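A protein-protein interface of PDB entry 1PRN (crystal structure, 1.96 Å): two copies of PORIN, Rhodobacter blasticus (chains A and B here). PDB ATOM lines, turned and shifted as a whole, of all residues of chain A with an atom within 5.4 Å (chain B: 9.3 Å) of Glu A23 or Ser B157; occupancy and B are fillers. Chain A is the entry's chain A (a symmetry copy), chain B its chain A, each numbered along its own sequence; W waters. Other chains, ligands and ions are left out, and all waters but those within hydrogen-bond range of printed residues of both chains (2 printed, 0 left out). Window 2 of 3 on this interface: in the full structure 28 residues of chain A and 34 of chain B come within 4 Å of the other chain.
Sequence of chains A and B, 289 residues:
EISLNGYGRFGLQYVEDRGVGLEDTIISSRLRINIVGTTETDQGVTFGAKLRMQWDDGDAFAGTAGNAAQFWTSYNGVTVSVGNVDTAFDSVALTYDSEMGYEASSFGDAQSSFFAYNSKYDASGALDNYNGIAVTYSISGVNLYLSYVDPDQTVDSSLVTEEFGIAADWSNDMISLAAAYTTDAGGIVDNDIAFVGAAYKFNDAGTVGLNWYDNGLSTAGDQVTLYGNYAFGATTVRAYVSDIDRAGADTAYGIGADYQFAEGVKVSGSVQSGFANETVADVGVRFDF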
ATOM      1  N   ARG A  18       0.156 -23.204  30.690  1.00  0.00           N
ATOM      2  CA  ARG A  18       1.002 -24.317  31.132  1.00  0.00           C
ATOM      3  C   ARG A  18       1.760 -24.056  32.435  1.00  0.00           C
ATOM      4  O   ARG A  18       2.005 -24.975  33.225  1.00  0.00           O
ATOM      5  CB  ARG A  18       1.988 -24.676  30.019  1.00  0.00           C
ATOM      6  CG  ARG A  18       2.731 -25.915  30.251  1.00  0.00           C
ATOM      7  CD  ARG A  18       3.791 -26.030  29.184  1.00  0.00           C
ATOM      8  NE  ARG A  18       3.267 -26.316  27.847  1.00  0.00           N
ATOM      9  CZ  ARG A  18       3.084 -27.543  27.345  1.00  0.00           C
ATOM     10  NH1 ARG A  18       3.356 -28.619  28.066  1.00  0.00           N
ATOM     11  NH2 ARG A  18       2.703 -27.699  26.081  1.00  0.00           N
ATOM     12  N   GLY A  19       2.176 -22.813  32.637  1.00  0.00           N
ATOM     13  CA  GLY A  19       2.905 -22.472  33.839  1.00  0.00           C
ATOM     14  C   GLY A  19       3.531 -21.104  33.711  1.00  0.00           C
ATOM     15  O   GLY A  19       3.668 -20.572  32.607  1.00  0.00           O
ATOM     16  N   GLY A  21       6.185 -18.504  33.230  1.00  0.00           N
ATOM     17  CA  GLY A  21       7.487 -18.515  32.583  1.00  0.00           C
ATOM     18  C   GLY A  21       7.644 -19.617  31.546  1.00  0.00           C
ATOM     19  O   GLY A  21       8.714 -19.740  30.937  1.00  0.00           O
ATOM     20  N   LEU A  22       6.591 -20.416  31.357  1.00  0.00           N
ATOM     21  CA  LEU A  22       6.588 -21.513  30.397  1.00  0.00           C
ATOM     22  C   LEU A  22       5.848 -21.166  29.125  1.00  0.00           C
ATOM     23  O   LEU A  22       4.929 -20.345  29.104  1.00  0.00           O
ATOM     24  CB  LEU A  22       5.940 -22.767  30.983  1.00  0.00           C
ATOM     25  CG  LEU A  22       6.560 -23.372  32.229  1.00  0.00           C
ATOM     26  CD1 LEU A  22       5.782 -24.614  32.581  1.00  0.00           C
ATOM     27  CD2 LEU A  22       8.025 -23.702  32.000  1.00  0.00           C
ATOM     28  N   GLU A  23       6.230 -21.852  28.066  1.00  0.00           N
ATOM     29  CA  GLU A  23       5.631 -21.673  26.763  1.00  0.00           C
ATOM     30  C   GLU A  23       4.453 -22.644  26.729  1.00  0.00           C
ATOM     31  O   GLU A  23       4.595 -23.808  27.107  1.00  0.00           O
ATOM     32  CB  GLU A  23       6.663 -22.039  25.704  1.00  0.00           C
ATOM     33  CG  GLU A  23       6.454 -21.417  24.369  1.00  0.00           C
ATOM     34  CD  GLU A  23       6.633 -19.915  24.387  1.00  0.00           C
ATOM     35  OE1 GLU A  23       7.786 -19.438  24.355  1.00  0.00           O
ATOM     36  OE2 GLU A  23       5.611 -19.206  24.428  1.00  0.00           O
ATOM     37  N   ASP A  24       3.286 -22.166  26.323  1.00  0.00           N
ATOM     38  CA  ASP A  24       2.105 -23.020  26.249  1.00  0.00           C
ATOM     39  C   ASP A  24       2.206 -24.086  25.166  1.00  0.00           C
ATOM     40  O   ASP A  24       1.648 -25.175  25.303  1.00  0.00           O
ATOM     41  CB  ASP A  24       0.852 -22.183  25.988  1.00  0.00           C
ATOM     42  CG  ASP A  24       0.368 -21.460  27.210  1.00  0.00           C
ATOM     43  OD1 ASP A  24       0.909 -21.699  28.306  1.00  0.00           O
ATOM     44  OD2 ASP A  24      -0.573 -20.661  27.078  1.00  0.00           O
ATOM     45  N   THR A  25       2.851 -23.730  24.065  1.00  0.00           N
ATOM     46  CA  THR A  25       3.019 -24.627  22.935  1.00  0.00           C
ATOM     47  C   THR A  25       4.466 -25.059  22.767  1.00  0.00           C
ATOM     48  O   THR A  25       5.363 -24.224  22.732  1.00  0.00           O
ATOM     49  CB  THR A  25       2.587 -23.948  21.618  1.00  0.00           C
ATOM     50  OG1 THR A  25       1.214 -23.547  21.719  1.00  0.00           O
ATOM     51  CG2 THR A  25       2.736 -24.909  20.425  1.00  0.00           C
ATOM     52  N   ILE A  26       4.694 -26.364  22.667  1.00  0.00           N
ATOM     53  CA  ILE A  26       6.040 -26.883  22.446  1.00  0.00           C
ATOM     54  C   ILE A  26       5.979 -27.932  21.321  1.00  0.00           C
ATOM     55  O   ILE A  26       4.901 -28.273  20.848  1.00  0.00           O
ATOM     56  CB  ILE A  26       6.623 -27.544  23.718  1.00  0.00           C
ATOM     57  CG1 ILE A  26       5.786 -28.756  24.105  1.00  0.00           C
ATOM     58  CG2 ILE A  26       6.669 -26.545  24.874  1.00  0.00           C
ATOM     59  CD1 ILE A  26       6.416 -29.596  25.154  1.00  0.00           C
ATOM     60  N   TYR B 148      17.577 -23.293  13.088  1.00  0.00           N
ATOM     61  CA  TYR B 148      17.140 -22.511  14.222  1.00  0.00           C
ATOM     62  C   TYR B 148      17.183 -23.468  15.410  1.00  0.00           C
ATOM     63  O   TYR B 148      16.630 -24.558  15.359  1.00  0.00           O
ATOM     64  CB  TYR B 148      15.736 -21.997  13.962  1.00  0.00           C
ATOM     65  CG  TYR B 148      15.003 -21.587  15.198  1.00  0.00           C
ATOM     66  CD1 TYR B 148      15.174 -20.320  15.747  1.00  0.00           C
ATOM     67  CD2 TYR B 148      14.123 -22.476  15.823  1.00  0.00           C
ATOM     68  CE1 TYR B 148      14.479 -19.941  16.901  1.00  0.00           C
ATOM     69  CE2 TYR B 148      13.428 -22.120  16.967  1.00  0.00           C
ATOM     70  CZ  TYR B 148      13.606 -20.851  17.509  1.00  0.00           C
ATOM     71  OH  TYR B 148      12.921 -20.510  18.662  1.00  0.00           O
ATOM     72  N   VAL B 149      17.934 -23.108  16.439  1.00  0.00           N
ATOM     73  CA  VAL B 149      18.051 -23.961  17.611  1.00  0.00           C
ATOM     74  C   VAL B 149      17.628 -23.200  18.865  1.00  0.00           C
ATOM     75  O   VAL B 149      18.094 -22.089  19.133  1.00  0.00           O
ATOM     76  CB  VAL B 149      19.504 -24.493  17.790  1.00  0.00           C
ATOM     77  CG1 VAL B 149      19.581 -25.410  18.988  1.00  0.00           C
ATOM     78  CG2 VAL B 149      19.960 -25.240  16.548  1.00  0.00           C
ATOM     79  N   ASP B 150      16.680 -23.775  19.583  1.00  0.00           N
ATOM     80  CA  ASP B 150      16.197 -23.195  20.808  1.00  0.00           C
ATOM     81  C   ASP B 150      16.798 -24.085  21.899  1.00  0.00           C
ATOM     82  O   ASP B 150      16.413 -25.246  22.042  1.00  0.00           O
ATOM     83  CB  ASP B 150      14.681 -23.275  20.822  1.00  0.00           C
ATOM     84  CG  ASP B 150      14.069 -22.509  21.966  1.00  0.00           C
ATOM     85  OD1 ASP B 150      14.777 -22.258  22.964  1.00  0.00           O
ATOM     86  OD2 ASP B 150      12.869 -22.169  21.866  1.00  0.00           O
ATOM     87  N   PRO B 151      17.766 -23.558  22.659  1.00  0.00           N
ATOM     88  CA  PRO B 151      18.410 -24.340  23.732  1.00  0.00           C
ATOM     89  C   PRO B 151      17.490 -24.861  24.847  1.00  0.00           C
ATOM     90  O   PRO B 151      17.845 -25.809  25.558  1.00  0.00           O
ATOM     91  CB  PRO B 151      19.510 -23.395  24.213  1.00  0.00           C
ATOM     92  CG  PRO B 151      19.016 -22.038  23.850  1.00  0.00           C
ATOM     93  CD  PRO B 151      18.382 -22.234  22.524  1.00  0.00           C
ATOM     94  N   ASP B 152      16.334 -24.231  25.023  1.00  0.00           N
ATOM     95  CA  ASP B 152      15.347 -24.671  26.010  1.00  0.00           C
ATOM     96  C   ASP B 152      13.982 -24.202  25.511  1.00  0.00           C
ATOM     97  O   ASP B 152      13.531 -23.087  25.812  1.00  0.00           O
ATOM     98  CB  ASP B 152      15.632 -24.115  27.407  1.00  0.00           C
ATOM     99  CG  ASP B 152      14.758 -24.754  28.478  1.00  0.00           C
ATOM    100  OD1 ASP B 152      13.575 -25.061  28.205  1.00  0.00           O
ATOM    101  OD2 ASP B 152      15.244 -24.951  29.611  1.00  0.00           O
ATOM    102  N   GLN B 153      13.295 -25.090  24.803  1.00  0.00           N
ATOM    103  CA  GLN B 153      12.006 -24.774  24.216  1.00  0.00           C
ATOM    104  C   GLN B 153      10.823 -24.669  25.168  1.00  0.00           C
ATOM    105  O   GLN B 153       9.764 -24.205  24.775  1.00  0.00           O
ATOM    106  CB  GLN B 153      11.677 -25.785  23.113  1.00  0.00           C
ATOM    107  CG  GLN B 153      11.282 -27.200  23.644  1.00  0.00           C
ATOM    108  CD  GLN B 153      10.495 -28.004  22.637  1.00  0.00           C
ATOM    109  OE1 GLN B 153       9.917 -27.449  21.695  1.00  0.00           O
ATOM    110  NE2 GLN B 153      10.427 -29.301  22.847  1.00  0.00           N
ATOM    111  N   THR B 154      10.973 -25.127  26.402  1.00  0.00           N
ATOM    112  CA  THR B 154       9.867 -25.073  27.351  1.00  0.00           C
ATOM    113  C   THR B 154       9.751 -23.703  28.025  1.00  0.00           C
ATOM    114  O   THR B 154       8.686 -23.329  28.511  1.00  0.00           O
ATOM    115  CB  THR B 154      10.020 -26.153  28.450  1.00  0.00           C
ATOM    116  OG1 THR B 154      11.197 -25.876  29.210  1.00  0.00           O
ATOM    117  CG2 THR B 154      10.156 -27.557  27.849  1.00  0.00           C
ATOM    118  N   VAL B 155      10.854 -22.966  28.060  1.00  0.00           N
ATOM    119  CA  VAL B 155      10.911 -21.649  28.689  1.00  0.00           C
ATOM    120  C   VAL B 155      10.505 -20.540  27.738  1.00  0.00           C
ATOM    121  O   VAL B 155      10.748 -20.615  26.534  1.00  0.00           O
ATOM    122  CB  VAL B 155      12.335 -21.377  29.225  1.00  0.00           C
ATOM    123  CG1 VAL B 155      12.543 -19.910  29.506  1.00  0.00           C
ATOM    124  CG2 VAL B 155      12.558 -22.189  30.479  1.00  0.00           C
ATOM    125  N   ASP B 156       9.881 -19.511  28.285  1.00  0.00           N
ATOM    126  CA  ASP B 156       9.449 -18.384  27.483  1.00  0.00           C
ATOM    127  C   ASP B 156      10.616 -17.917  26.616  1.00  0.00           C
ATOM    128  O   ASP B 156      11.712 -17.685  27.121  1.00  0.00           O
ATOM    129  CB  ASP B 156       9.005 -17.256  28.400  1.00  0.00           C
ATOM    130  CG  ASP B 156       8.020 -16.336  27.738  1.00  0.00           C
ATOM    131  OD1 ASP B 156       8.412 -15.616  26.786  1.00  0.00           O
ATOM    132  OD2 ASP B 156       6.840 -16.354  28.162  1.00  0.00           O
ATOM    133  N   SER B 157      10.369 -17.783  25.318  1.00  0.00           N
ATOM    134  CA  SER B 157      11.376 -17.373  24.336  1.00  0.00           C
ATOM    135  C   SER B 157      12.208 -16.139  24.667  1.00  0.00           C
ATOM    136  O   SER B 157      13.425 -16.134  24.473  1.00  0.00           O
ATOM    137  CB  SER B 157      10.715 -17.154  22.982  1.00  0.00           C
ATOM    138  OG  SER B 157       9.694 -18.101  22.771  1.00  0.00           O
ATOM    139  N   SER B 158      11.553 -15.083  25.135  1.00  0.00           N
ATOM    140  CA  SER B 158      12.246 -13.843  25.477  1.00  0.00           C
ATOM    141  C   SER B 158      13.328 -14.045  26.541  1.00  0.00           C
ATOM    142  O   SER B 158      14.218 -13.204  26.707  1.00  0.00           O
ATOM    143  CB  SER B 158      11.234 -12.799  25.950  1.00  0.00           C
ATOM    144  OG  SER B 158      10.399 -13.336  26.969  1.00  0.00           O
ATOM    145  N   LEU B 159      13.260 -15.166  27.247  1.00  0.00           N
ATOM    146  CA  LEU B 159      14.228 -15.454  28.286  1.00  0.00           C
ATOM    147  C   LEU B 159      15.419 -16.260  27.773  1.00  0.00           C
ATOM    148  O   LEU B 159      16.456 -16.315  28.434  1.00  0.00           O
ATOM    149  CB  LEU B 159      13.554 -16.214  29.432  1.00  0.00           C
ATOM    150  CG  LEU B 159      12.245 -15.650  30.004  1.00  0.00           C
ATOM    151  CD1 LEU B 159      11.718 -16.570  31.099  1.00  0.00           C
ATOM    152  CD2 LEU B 159      12.457 -14.239  30.536  1.00  0.00           C
ATOM    153  N   VAL B 160      15.273 -16.912  26.620  1.00  0.00           N
ATOM    154  CA  VAL B 160      16.368 -17.723  26.085  1.00  0.00           C
ATOM    155  C   VAL B 160      16.922 -17.124  24.807  1.00  0.00           C
ATOM    156  O   VAL B 160      16.227 -16.379  24.111  1.00  0.00           O
ATOM    157  CB  VAL B 160      15.940 -19.210  25.815  1.00  0.00           C
ATOM    158  CG1 VAL B 160      15.159 -19.769  26.987  1.00  0.00           C
ATOM    159  CG2 VAL B 160      15.123 -19.313  24.560  1.00  0.00           C
ATOM    160  N   THR B 161      18.173 -17.449  24.502  1.00  0.00           N
ATOM    161  CA  THR B 161      18.842 -16.972  23.288  1.00  0.00           C
ATOM    162  C   THR B 161      18.844 -18.107  22.264  1.00  0.00           C
ATOM    163  O   THR B 161      19.429 -19.164  22.503  1.00  0.00           O
ATOM    164  CB  THR B 161      20.313 -16.598  23.576  1.00  0.00           C
ATOM    165  OG1 THR B 161      20.365 -15.635  24.634  1.00  0.00           O
ATOM    166  CG2 THR B 161      20.992 -16.030  22.336  1.00  0.00           C
ATOM    167  N   GLU B 162      18.184 -17.902  21.135  1.00  0.00           N
ATOM    168  CA  GLU B 162      18.152 -18.923  20.101  1.00  0.00           C
ATOM    169  C   GLU B 162      19.181 -18.622  19.036  1.00  0.00           C
ATOM    170  O   GLU B 162      19.474 -17.459  18.748  1.00  0.00           O
ATOM    171  CB  GLU B 162      16.774 -19.021  19.464  1.00  0.00           C
ATOM    172  CG  GLU B 162      15.714 -19.428  20.407  1.00  0.00           C
ATOM    173  CD  GLU B 162      14.956 -18.254  21.000  1.00  0.00           C
ATOM    174  OE1 GLU B 162      15.297 -17.084  20.728  1.00  0.00           O
ATOM    175  OE2 GLU B 162      13.988 -18.505  21.744  1.00  0.00           O
HETATM  176  O   HOH W   1       6.681 -25.308  28.237  1.00  0.00           O
HETATM  177  O   HOH W   2       8.635 -23.376  22.353  1.00  0.00           O
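The backbone carbonyl oxygen (O) of Thr B154 lies within hydrogen-bond range of the backbone NH (N) of Glu A23.
The backbone carbonyl oxygen (O) of Gly A21 sits at hydrogen-bond distance from the backbone NH (N) of Asp B156, at 2.9 Å.
The side-chain carboxylate of Glu A23 sits at hydrogen-bond distance from the side-chain hydroxyl of Ser B157 (2.8 Å).
The side-chain carboxylate (OD1) of Asp B152 sits at hydrogen-bond distance from the side-chain hydroxyl (OG1) of Thr B154.
The side-chain carboxylate (OD1) of Asp B152 sits at hydrogen-bond distance from the backbone NH (N) of Val B155, 3.4 Å away.
The side-chain hydroxyl of Ser B158 lies within hydrogen-bond range of the side-chain carboxylate of Asp B156.
NE of Arg A18 is in hydrogen-bond range of O of Glu A23 (2.9 Å).
Gly A21 touches Val B155 (O to CA, 3.7 Å).
CA of Leu A22 touches O of Thr B154, at 3.4 Å.
CB of Glu A23 touches O of Gln B153, at 3.9 Å.
O of Val B155 touches OE1 of Glu A23 (3.9 Å).
OE1 of Glu A23 touches CA of Asp B156, 3.7 Å away.
Ile A26 touches Gln B153 (CB to OE1, 3.9 Å).
Of the printed residues of chain B, Gly A21 touches Val B155 (3.7 Å) and Asp B156 (2.9 Å).
Of the printed residues of chain B, Glu A23 touches Gln B153, Thr B154, Val B155, Asp B156 and Ser B157.
Asp A24 touches none of the printed residues of chain B.
Of the printed residues of chain A, Gln B153 touches Glu A23 (3.9 Å) and Ile A26 (3.9 Å).
Of the printed residues of chain A, Val B155 touches Gly A21 (3.7 Å) and Glu A23 (3.9 Å).
Ser B157 touches just one residue of chain A: Glu A23.
Thr B161 touches none of the printed residues of chain A.
The nearest residue of chain B that does not touch Glu A23 is Ser B158 (5.8 Å).
The nearest printed residue of chain A that does not touch Ser B157 is Gly A21 (6.2 Å).
Of the 8 printed residues of chain A, 4 touch a printed residue of chain B.
Among the printed residues, 9 pairs touch across the chains.
Among the printed residues, no Asp or Glu carboxylate lies within 4 Å of a Lys or Arg side-chain nitrogen of the other chain.
No position is printed for both chains.
Water W2 lies within hydrogen-bond range of O of Gln B153 and O of Thr A25.
Water W1 lies within hydrogen-bond range of O of Glu A23 (2.8 Å) and O of Thr B154 (2.8 Å).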
